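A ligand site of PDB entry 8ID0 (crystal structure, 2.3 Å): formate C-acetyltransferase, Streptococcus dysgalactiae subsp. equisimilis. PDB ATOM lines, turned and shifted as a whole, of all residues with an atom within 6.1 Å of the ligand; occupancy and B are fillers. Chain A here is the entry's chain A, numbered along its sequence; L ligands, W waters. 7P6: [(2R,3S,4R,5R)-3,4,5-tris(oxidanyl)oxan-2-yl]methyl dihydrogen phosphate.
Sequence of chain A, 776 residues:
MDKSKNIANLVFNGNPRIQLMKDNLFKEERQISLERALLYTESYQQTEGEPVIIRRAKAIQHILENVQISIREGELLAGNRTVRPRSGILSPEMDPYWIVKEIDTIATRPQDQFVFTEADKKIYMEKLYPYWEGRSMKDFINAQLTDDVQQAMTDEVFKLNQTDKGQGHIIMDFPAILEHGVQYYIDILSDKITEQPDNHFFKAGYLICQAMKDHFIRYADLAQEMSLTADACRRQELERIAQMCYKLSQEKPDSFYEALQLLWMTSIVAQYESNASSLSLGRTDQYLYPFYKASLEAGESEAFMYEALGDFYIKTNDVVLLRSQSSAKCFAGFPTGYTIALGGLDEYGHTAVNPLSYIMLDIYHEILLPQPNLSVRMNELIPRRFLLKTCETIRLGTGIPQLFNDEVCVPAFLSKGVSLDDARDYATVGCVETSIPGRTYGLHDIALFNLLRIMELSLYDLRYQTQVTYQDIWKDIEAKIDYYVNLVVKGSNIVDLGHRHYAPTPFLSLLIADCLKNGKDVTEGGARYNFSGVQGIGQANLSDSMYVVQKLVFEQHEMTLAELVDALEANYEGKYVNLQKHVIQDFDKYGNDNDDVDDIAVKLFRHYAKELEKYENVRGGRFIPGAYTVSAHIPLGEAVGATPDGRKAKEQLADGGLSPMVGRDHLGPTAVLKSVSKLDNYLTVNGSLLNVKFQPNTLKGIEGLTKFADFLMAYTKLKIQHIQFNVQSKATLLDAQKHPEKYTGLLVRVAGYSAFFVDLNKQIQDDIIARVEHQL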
ATOM      1  N   ASN A 161      -1.850  -3.597 -34.092  1.00  0.00           N
ATOM      2  CA  ASN A 161      -1.872  -4.749 -33.198  1.00  0.00           C
ATOM      3  C   ASN A 161      -3.300  -5.017 -32.725  1.00  0.00           C
ATOM      4  O   ASN A 161      -4.211  -4.209 -32.941  1.00  0.00           O
ATOM      5  CB  ASN A 161      -0.936  -4.524 -31.998  1.00  0.00           C
ATOM      6  CG  ASN A 161       0.489  -4.229 -32.423  1.00  0.00           C
ATOM      7  OD1 ASN A 161       1.020  -4.878 -33.313  1.00  0.00           O
ATOM      8  ND2 ASN A 161       1.114  -3.233 -31.785  1.00  0.00           N
ATOM      9  N   GLN A 162      -3.467  -6.167 -32.069  1.00  0.00           N
ATOM     10  CA  GLN A 162      -4.774  -6.642 -31.573  1.00  0.00           C
ATOM     11  C   GLN A 162      -5.878  -6.522 -32.633  1.00  0.00           C
ATOM     12  O   GLN A 162      -7.030  -6.182 -32.336  1.00  0.00           O
ATOM     13  CB  GLN A 162      -5.181  -5.908 -30.294  1.00  0.00           C
ATOM     14  CG  GLN A 162      -4.219  -6.069 -29.126  1.00  0.00           C
ATOM     15  CD  GLN A 162      -3.213  -4.949 -29.075  1.00  0.00           C
ATOM     16  OE1 GLN A 162      -3.546  -3.793 -29.350  1.00  0.00           O
ATOM     17  NE2 GLN A 162      -1.973  -5.274 -28.722  1.00  0.00           N
ATOM     18  N   LYS A 165      -7.230 -10.604 -31.809  1.00  0.00           N
ATOM     19  CA  LYS A 165      -7.145 -11.109 -30.448  1.00  0.00           C
ATOM     20  C   LYS A 165      -7.703 -10.038 -29.527  1.00  0.00           C
ATOM     21  O   LYS A 165      -7.899  -8.893 -29.925  1.00  0.00           O
ATOM     22  CB  LYS A 165      -5.701 -11.471 -30.074  1.00  0.00           C
ATOM     23  CG  LYS A 165      -4.724 -10.293 -30.106  1.00  0.00           C
ATOM     24  CD  LYS A 165      -3.334 -10.689 -29.623  1.00  0.00           C
ATOM     25  CE  LYS A 165      -2.614 -11.598 -30.630  1.00  0.00           C
ATOM     26  NZ  LYS A 165      -2.047 -10.890 -31.828  1.00  0.00           N
ATOM     27  N   GLY A 166      -7.933 -10.434 -28.279  1.00  0.00           N
ATOM     28  CA  GLY A 166      -8.417  -9.494 -27.290  1.00  0.00           C
ATOM     29  C   GLY A 166      -7.442  -8.351 -27.071  1.00  0.00           C
ATOM     30  O   GLY A 166      -6.253  -8.418 -27.415  1.00  0.00           O
ATOM     31  N   GLN A 167      -7.969  -7.276 -26.491  1.00  0.00           N
ATOM     32  CA  GLN A 167      -7.200  -6.048 -26.342  1.00  0.00           C
ATOM     33  C   GLN A 167      -6.247  -6.144 -25.144  1.00  0.00           C
ATOM     34  O   GLN A 167      -5.038  -5.965 -25.297  1.00  0.00           O
ATOM     35  CB  GLN A 167      -8.155  -4.859 -26.218  1.00  0.00           C
ATOM     36  CG  GLN A 167      -7.529  -3.588 -25.701  1.00  0.00           C
ATOM     37  CD  GLN A 167      -6.314  -3.134 -26.518  1.00  0.00           C
ATOM     38  OE1 GLN A 167      -5.409  -2.493 -25.976  1.00  0.00           O
ATOM     39  NE2 GLN A 167      -6.304  -3.420 -27.823  1.00  0.00           N
ATOM     40  N   HIS A 169      -4.000  -5.281 -22.033  1.00  0.00           N
ATOM     41  CA  HIS A 169      -3.223  -4.073 -21.754  1.00  0.00           C
ATOM     42  C   HIS A 169      -3.979  -3.133 -20.828  1.00  0.00           C
ATOM     43  O   HIS A 169      -4.187  -1.952 -21.123  1.00  0.00           O
ATOM     44  CB  HIS A 169      -2.844  -3.354 -23.054  1.00  0.00           C
ATOM     45  CG  HIS A 169      -1.996  -4.187 -23.982  1.00  0.00           C
ATOM     46  ND1 HIS A 169      -2.524  -5.186 -24.776  1.00  0.00           N
ATOM     47  CD2 HIS A 169      -0.668  -4.145 -24.257  1.00  0.00           C
ATOM     48  CE1 HIS A 169      -1.559  -5.735 -25.485  1.00  0.00           C
ATOM     49  NE2 HIS A 169      -0.424  -5.127 -25.197  1.00  0.00           N
ATOM     50  N   ALA A 276      -6.516 -12.119 -23.350  1.00  0.00           N
ATOM     51  CA  ALA A 276      -5.604 -11.141 -23.896  1.00  0.00           C
ATOM     52  C   ALA A 276      -4.315 -11.082 -23.078  1.00  0.00           C
ATOM     53  O   ALA A 276      -4.213 -11.654 -21.981  1.00  0.00           O
ATOM     54  CB  ALA A 276      -6.255  -9.749 -23.967  1.00  0.00           C
ATOM     55  N   SER A 277      -3.347 -10.360 -23.608  1.00  0.00           N
ATOM     56  CA  SER A 277      -2.090 -10.128 -22.912  1.00  0.00           C
ATOM     57  C   SER A 277      -2.218  -8.935 -21.977  1.00  0.00           C
ATOM     58  O   SER A 277      -3.032  -8.026 -22.184  1.00  0.00           O
ATOM     59  CB  SER A 277      -0.950  -9.876 -23.901  1.00  0.00           C
ATOM     60  OG  SER A 277      -0.989 -10.734 -25.023  1.00  0.00           O
ATOM     61  N   SER A 278      -1.394  -8.953 -20.933  1.00  0.00           N
ATOM     62  CA  SER A 278      -1.134  -7.770 -20.113  1.00  0.00           C
ATOM     63  C   SER A 278      -2.381  -7.298 -19.378  1.00  0.00           C
ATOM     64  O   SER A 278      -2.719  -6.112 -19.355  1.00  0.00           O
ATOM     65  CB  SER A 278      -0.545  -6.661 -20.957  1.00  0.00           C
ATOM     66  OG  SER A 278       0.622  -7.166 -21.570  1.00  0.00           O
ATOM     67  N   LEU A 321      -0.161 -16.653 -24.328  1.00  0.00           N
ATOM     68  CA  LEU A 321      -1.146 -16.257 -25.312  1.00  0.00           C
ATOM     69  C   LEU A 321      -0.756 -16.768 -26.694  1.00  0.00           C
ATOM     70  O   LEU A 321       0.428 -16.764 -27.069  1.00  0.00           O
ATOM     71  CB  LEU A 321      -1.362 -14.744 -25.298  1.00  0.00           C
ATOM     72  CG  LEU A 321      -1.922 -14.582 -23.882  1.00  0.00           C
ATOM     73  CD1 LEU A 321      -1.144 -13.571 -23.045  1.00  0.00           C
ATOM     74  CD2 LEU A 321      -3.421 -14.350 -23.846  1.00  0.00           C
ATOM     75  N   ARG A 323      -0.772 -16.726 -30.776  1.00  0.00           N
ATOM     76  CA  ARG A 323      -0.741 -15.690 -31.782  1.00  0.00           C
ATOM     77  C   ARG A 323      -0.248 -16.300 -33.069  1.00  0.00           C
ATOM     78  O   ARG A 323       0.283 -17.420 -33.094  1.00  0.00           O
ATOM     79  CB  ARG A 323       0.124 -14.490 -31.347  1.00  0.00           C
ATOM     80  CG  ARG A 323       1.642 -14.757 -31.316  1.00  0.00           C
ATOM     81  CD  ARG A 323       2.419 -13.532 -30.787  1.00  0.00           C
ATOM     82  NE  ARG A 323       2.092 -13.212 -29.392  1.00  0.00           N
ATOM     83  CZ  ARG A 323       1.436 -12.121 -29.000  1.00  0.00           C
ATOM     84  NH1 ARG A 323       1.040 -11.219 -29.902  1.00  0.00           N
ATOM     85  NH2 ARG A 323       1.184 -11.905 -27.710  1.00  0.00           N
ATOM     86  N   SER A 327       2.540 -12.449 -36.075  1.00  0.00           N
ATOM     87  CA  SER A 327       2.463 -11.766 -34.793  1.00  0.00           C
ATOM     88  C   SER A 327       3.594 -12.199 -33.863  1.00  0.00           C
ATOM     89  O   SER A 327       4.099 -11.386 -33.088  1.00  0.00           O
ATOM     90  CB  SER A 327       1.117 -12.016 -34.133  1.00  0.00           C
ATOM     91  OG  SER A 327       0.954 -11.224 -32.959  1.00  0.00           O
ATOM     92  N   PHE A 331       6.241 -10.218 -31.186  1.00  0.00           N
ATOM     93  CA  PHE A 331       5.936 -10.462 -29.781  1.00  0.00           C
ATOM     94  C   PHE A 331       6.312 -11.890 -29.384  1.00  0.00           C
ATOM     95  O   PHE A 331       5.492 -12.687 -28.907  1.00  0.00           O
ATOM     96  CB  PHE A 331       4.456 -10.158 -29.537  1.00  0.00           C
ATOM     97  CG  PHE A 331       4.013  -8.824 -30.117  1.00  0.00           C
ATOM     98  CD1 PHE A 331       4.652  -7.642 -29.731  1.00  0.00           C
ATOM     99  CD2 PHE A 331       2.973  -8.752 -31.037  1.00  0.00           C
ATOM    100  CE1 PHE A 331       4.266  -6.436 -30.250  1.00  0.00           C
ATOM    101  CE2 PHE A 331       2.564  -7.531 -31.544  1.00  0.00           C
ATOM    102  CZ  PHE A 331       3.208  -6.373 -31.160  1.00  0.00           C
ATOM    103  N   PRO A 335       5.322 -12.794 -24.009  1.00  0.00           N
ATOM    104  CA  PRO A 335       5.272 -11.618 -23.111  1.00  0.00           C
ATOM    105  C   PRO A 335       3.911 -11.446 -22.453  1.00  0.00           C
ATOM    106  O   PRO A 335       3.101 -10.573 -22.797  1.00  0.00           O
ATOM    107  CB  PRO A 335       5.614 -10.475 -24.061  1.00  0.00           C
ATOM    108  CG  PRO A 335       5.099 -10.940 -25.396  1.00  0.00           C
ATOM    109  CD  PRO A 335       5.380 -12.406 -25.433  1.00  0.00           C
ATOM    110  N   THR A 336       3.629 -12.284 -21.454  1.00  0.00           N
ATOM    111  CA  THR A 336       2.270 -12.381 -20.920  1.00  0.00           C
ATOM    112  C   THR A 336       1.840 -11.124 -20.155  1.00  0.00           C
ATOM    113  O   THR A 336       0.639 -10.791 -20.143  1.00  0.00           O
ATOM    114  CB  THR A 336       2.156 -13.628 -20.042  1.00  0.00           C
ATOM    115  OG1 THR A 336       2.321 -14.799 -20.868  1.00  0.00           O
ATOM    116  CG2 THR A 336       0.802 -13.705 -19.349  1.00  0.00           C
ATOM    117  N   GLY A 337       2.771 -10.430 -19.515  1.00  0.00           N
ATOM    118  CA  GLY A 337       2.424  -9.158 -18.914  1.00  0.00           C
ATOM    119  C   GLY A 337       1.672  -9.188 -17.593  1.00  0.00           C
ATOM    120  O   GLY A 337       0.877  -8.271 -17.335  1.00  0.00           O
ATOM    121  N   VAL A 429       1.640  -1.538 -17.398  1.00  0.00           N
ATOM    122  CA  VAL A 429       0.975  -2.568 -18.197  1.00  0.00           C
ATOM    123  C   VAL A 429       2.019  -3.256 -19.066  1.00  0.00           C
ATOM    124  O   VAL A 429       2.881  -2.600 -19.669  1.00  0.00           O
ATOM    125  CB  VAL A 429      -0.142  -1.957 -19.065  1.00  0.00           C
ATOM    126  CG1 VAL A 429      -0.513  -2.890 -20.203  1.00  0.00           C
ATOM    127  CG2 VAL A 429      -1.362  -1.650 -18.219  1.00  0.00           C
ATOM    128  N   GLY A 430       1.950  -4.579 -19.114  1.00  0.00           N
ATOM    129  CA  GLY A 430       2.730  -5.325 -20.100  1.00  0.00           C
ATOM    130  C   GLY A 430       4.220  -5.121 -19.902  1.00  0.00           C
ATOM    131  O   GLY A 430       4.775  -5.402 -18.830  1.00  0.00           O
ATOM    132  N   CYS A 431       4.884  -4.630 -20.945  1.00  0.00           N
ATOM    133  CA  CYS A 431       6.342  -4.453 -20.898  1.00  0.00           C
ATOM    134  C   CYS A 431       6.723  -3.191 -20.141  1.00  0.00           C
ATOM    135  O   CYS A 431       7.236  -3.266 -19.017  1.00  0.00           O
ATOM    136  CB  CYS A 431       6.910  -4.398 -22.323  1.00  0.00           C
ATOM    137  SG  CYS A 431       6.847  -5.979 -23.223  1.00  0.00           S
ATOM    138  N   VAL A 432       6.457  -2.022 -20.731  1.00  0.00           N
ATOM    139  CA  VAL A 432       6.903  -0.739 -20.198  1.00  0.00           C
ATOM    140  C   VAL A 432       5.787   0.290 -20.279  1.00  0.00           C
ATOM    141  O   VAL A 432       6.002   1.469 -20.020  1.00  0.00           O
ATOM    142  CB  VAL A 432       8.139  -0.218 -20.951  1.00  0.00           C
ATOM    143  CG1 VAL A 432       9.333  -1.115 -20.720  1.00  0.00           C
ATOM    144  CG2 VAL A 432       7.843  -0.103 -22.446  1.00  0.00           C
ATOM    145  N   GLU A 433       4.579  -0.144 -20.644  1.00  0.00           N
ATOM    146  CA  GLU A 433       3.459   0.787 -20.846  1.00  0.00           C
ATOM    147  C   GLU A 433       2.945   1.285 -19.492  1.00  0.00           C
ATOM    148  O   GLU A 433       1.950   0.820 -18.944  1.00  0.00           O
ATOM    149  CB  GLU A 433       2.358   0.120 -21.677  1.00  0.00           C
ATOM    150  CG  GLU A 433       2.863  -0.538 -22.965  1.00  0.00           C
ATOM    151  CD  GLU A 433       3.033  -2.052 -22.812  1.00  0.00           C
ATOM    152  OE1 GLU A 433       4.174  -2.535 -22.627  1.00  0.00           O
ATOM    153  OE2 GLU A 433       2.005  -2.763 -22.881  1.00  0.00           O
ATOM    154  N   HIS A 444      -2.463   0.457 -24.967  1.00  0.00           N
ATOM    155  CA  HIS A 444      -1.053   0.705 -24.684  1.00  0.00           C
ATOM    156  C   HIS A 444      -0.084   0.092 -25.679  1.00  0.00           C
ATOM    157  O   HIS A 444       1.093   0.451 -25.656  1.00  0.00           O
ATOM    158  CB  HIS A 444      -0.722   0.211 -23.295  1.00  0.00           C
ATOM    159  CG  HIS A 444      -1.224   1.127 -22.223  1.00  0.00           C
ATOM    160  ND1 HIS A 444      -0.863   2.448 -22.158  1.00  0.00           N
ATOM    161  CD2 HIS A 444      -2.075   0.905 -21.194  1.00  0.00           C
ATOM    162  CE1 HIS A 444      -1.449   3.009 -21.104  1.00  0.00           C
ATOM    163  NE2 HIS A 444      -2.190   2.094 -20.506  1.00  0.00           N
ATOM    164  N   ASP A 445      -0.527  -0.833 -26.531  1.00  0.00           N
ATOM    165  CA  ASP A 445       0.324  -1.257 -27.644  1.00  0.00           C
ATOM    166  C   ASP A 445      -0.521  -1.422 -28.898  1.00  0.00           C
ATOM    167  O   ASP A 445      -0.604  -2.492 -29.498  1.00  0.00           O
ATOM    168  CB  ASP A 445       1.099  -2.537 -27.358  1.00  0.00           C
ATOM    169  CG  ASP A 445       2.204  -2.756 -28.385  1.00  0.00           C
ATOM    170  OD1 ASP A 445       2.406  -1.838 -29.229  1.00  0.00           O
ATOM    171  OD2 ASP A 445       2.874  -3.821 -28.370  1.00  0.00           O
ATOM    172  N   TYR A 628       9.245   1.672 -27.460  1.00  0.00           N
ATOM    173  CA  TYR A 628       9.617   0.308 -27.100  1.00  0.00           C
ATOM    174  C   TYR A 628       9.291  -0.605 -28.280  1.00  0.00           C
ATOM    175  O   TYR A 628       8.505  -0.258 -29.158  1.00  0.00           O
ATOM    176  CB  TYR A 628       8.916  -0.151 -25.816  1.00  0.00           C
ATOM    177  CG  TYR A 628       7.408  -0.377 -25.902  1.00  0.00           C
ATOM    178  CD1 TYR A 628       6.889  -1.576 -26.371  1.00  0.00           C
ATOM    179  CD2 TYR A 628       6.509   0.600 -25.465  1.00  0.00           C
ATOM    180  CE1 TYR A 628       5.516  -1.806 -26.437  1.00  0.00           C
ATOM    181  CE2 TYR A 628       5.126   0.380 -25.528  1.00  0.00           C
ATOM    182  CZ  TYR A 628       4.647  -0.825 -26.019  1.00  0.00           C
ATOM    183  OH  TYR A 628       3.303  -1.093 -26.098  1.00  0.00           O
ATOM    184  N   VAL A 630       9.243  -4.512 -27.948  1.00  0.00           N
ATOM    185  CA  VAL A 630       9.088  -5.948 -27.716  1.00  0.00           C
ATOM    186  C   VAL A 630      10.148  -6.618 -28.589  1.00  0.00           C
ATOM    187  O   VAL A 630      11.311  -6.164 -28.613  1.00  0.00           O
ATOM    188  CB  VAL A 630       7.668  -6.451 -28.007  1.00  0.00           C
ATOM    189  CG1 VAL A 630       7.427  -7.775 -27.292  1.00  0.00           C
ATOM    190  CG2 VAL A 630       6.626  -5.433 -27.523  1.00  0.00           C
HETATM  191  C01 7P6 L   1       2.633  -6.851 -26.662  1.00  0.00           C
HETATM  192  C02 7P6 L   1       2.182  -7.685 -25.466  1.00  0.00           C
HETATM  193  C03 7P6 L   1       3.218  -7.309 -24.397  1.00  0.00           C
HETATM  194  C04 7P6 L   1       3.267  -5.787 -24.164  1.00  0.00           C
HETATM  195  C05 7P6 L   1       3.312  -4.965 -25.454  1.00  0.00           C
HETATM  196  C07 7P6 L   1       1.865  -7.164 -27.943  1.00  0.00           C
HETATM  197  O06 7P6 L   1       2.449  -5.473 -26.426  1.00  0.00           O
HETATM  198  O08 7P6 L   1       2.334  -9.042 -25.718  1.00  0.00           O
HETATM  199  O09 7P6 L   1       2.979  -7.893 -23.148  1.00  0.00           O
HETATM  200  O10 7P6 L   1       2.126  -5.431 -23.429  1.00  0.00           O
HETATM  201  O11 7P6 L   1       0.506  -6.999 -27.666  1.00  0.00           O
HETATM  202  O13 7P6 L   1       0.019  -9.447 -26.865  1.00  0.00           O
HETATM  203  O14 7P6 L   1      -0.268  -8.786 -29.258  1.00  0.00           O
HETATM  204  O15 7P6 L   1      -1.882  -8.006 -27.523  1.00  0.00           O
HETATM  205  P12 7P6 L   1      -0.435  -8.343 -27.811  1.00  0.00           P
HETATM  206  O   HOH W   1      -1.375  -8.000 -31.687  1.00  0.00           O
HETATM  207  O   HOH W   2       5.075  -7.885 -21.209  1.00  0.00           O
HETATM  208  O   HOH W   3       1.432 -12.186 -24.669  1.00  0.00           O
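Residues that only touch the ligand: Phe 331, Gly 430, Cys 431, Tyr 628 and Val 630.
Hydrophobic or aromatic side chains within 4 Å of the ligand: His 169, Phe 331, Pro 335, Tyr 628 and Val 630.
14 residues have an atom within 4 Å of the ligand: Gln 162, Lys 165, His 169, Ser 277, Ser 278, Arg 323, Phe 331, Pro 335, Gly 430, Cys 431, Glu 433, Asp 445, Tyr 628 and Val 630.
The nearest printed residue that does not touch the ligand is Gln 167 (4.4 Å).
Water W1 lies within hydrogen-bond range of an oxygen (O14) of the ligand (2.8 Å), the backbone NH (N) of Gln 162 (2.8 Å) and the side-chain amino group (NZ) of Lys 165 (3.0 Å).
Water W2 lies within hydrogen-bond range of O09 of the ligand (2.9 Å), N of Cys 431 (3.3 Å) and O of Gly 430 (3.5 Å).
Water W3 lies within hydrogen-bond range of OG of Ser 277 (2.8 Å), O of Pro 335 (3.0 Å), NH2 of Arg 323 (3.1 Å) and O08 of the ligand (3.4 Å).
The side-chain hydroxyl (OG) of Ser 327 lies within hydrogen-bond range of the guanidinium group (NH1) of Arg 323.
OE1 of Gln 162 is in hydrogen-bond range of NE2 of Gln 167 (3.2 Å).
The backbone carbonyl oxygen of Gln 167 is in hydrogen-bond range of a ring nitrogen (ND1) of His 169, 2.7 Å away.
N of Ser 278 lies within hydrogen-bond range of O of Thr 336, at 2.9 Å.
The side-chain hydroxyl (OH) of Tyr 628 is in hydrogen-bond range of the backbone carbonyl oxygen (O) of His 444 (2.7 Å).
The backbone NH (N) of His 169 lies within hydrogen-bond range of the backbone carbonyl oxygen (O) of Ser 278 (3.1 Å).
O of Asp 445 is in hydrogen-bond range of NE2 of Gln 162 (3.2 Å).
The backbone carbonyl oxygen of Ser 277 is in hydrogen-bond range of the backbone NH of His 169, at 2.9 Å.
O14 of the ligand is in salt-bridge range of NZ of Lys 165.
O09 of the ligand sits at hydrogen-bond distance from OG of Ser 278, 2.9 Å away.
The side-chain carboxylate of Glu 433 sits at hydrogen-bond distance from an oxygen (O10) of the ligand, at 2.7 Å.
NE2 of His 169 is in hydrogen-bond range of O10 of the ligand (3.1 Å).
O13 of the ligand sits at hydrogen-bond distance from OG of Ser 277.
NE2 of Gln 162 sits at hydrogen-bond distance from O15 of the ligand (3.0 Å).
O14 of the ligand is in salt-bridge range of NH1 of Arg 323 (2.8 Å).
The backbone carbonyl oxygen (O) of Pro 335 lies within hydrogen-bond range of an oxygen (O09) of the ligand.
OD2 of Asp 445 sits close to O06 of the ligand (2.6 Å).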
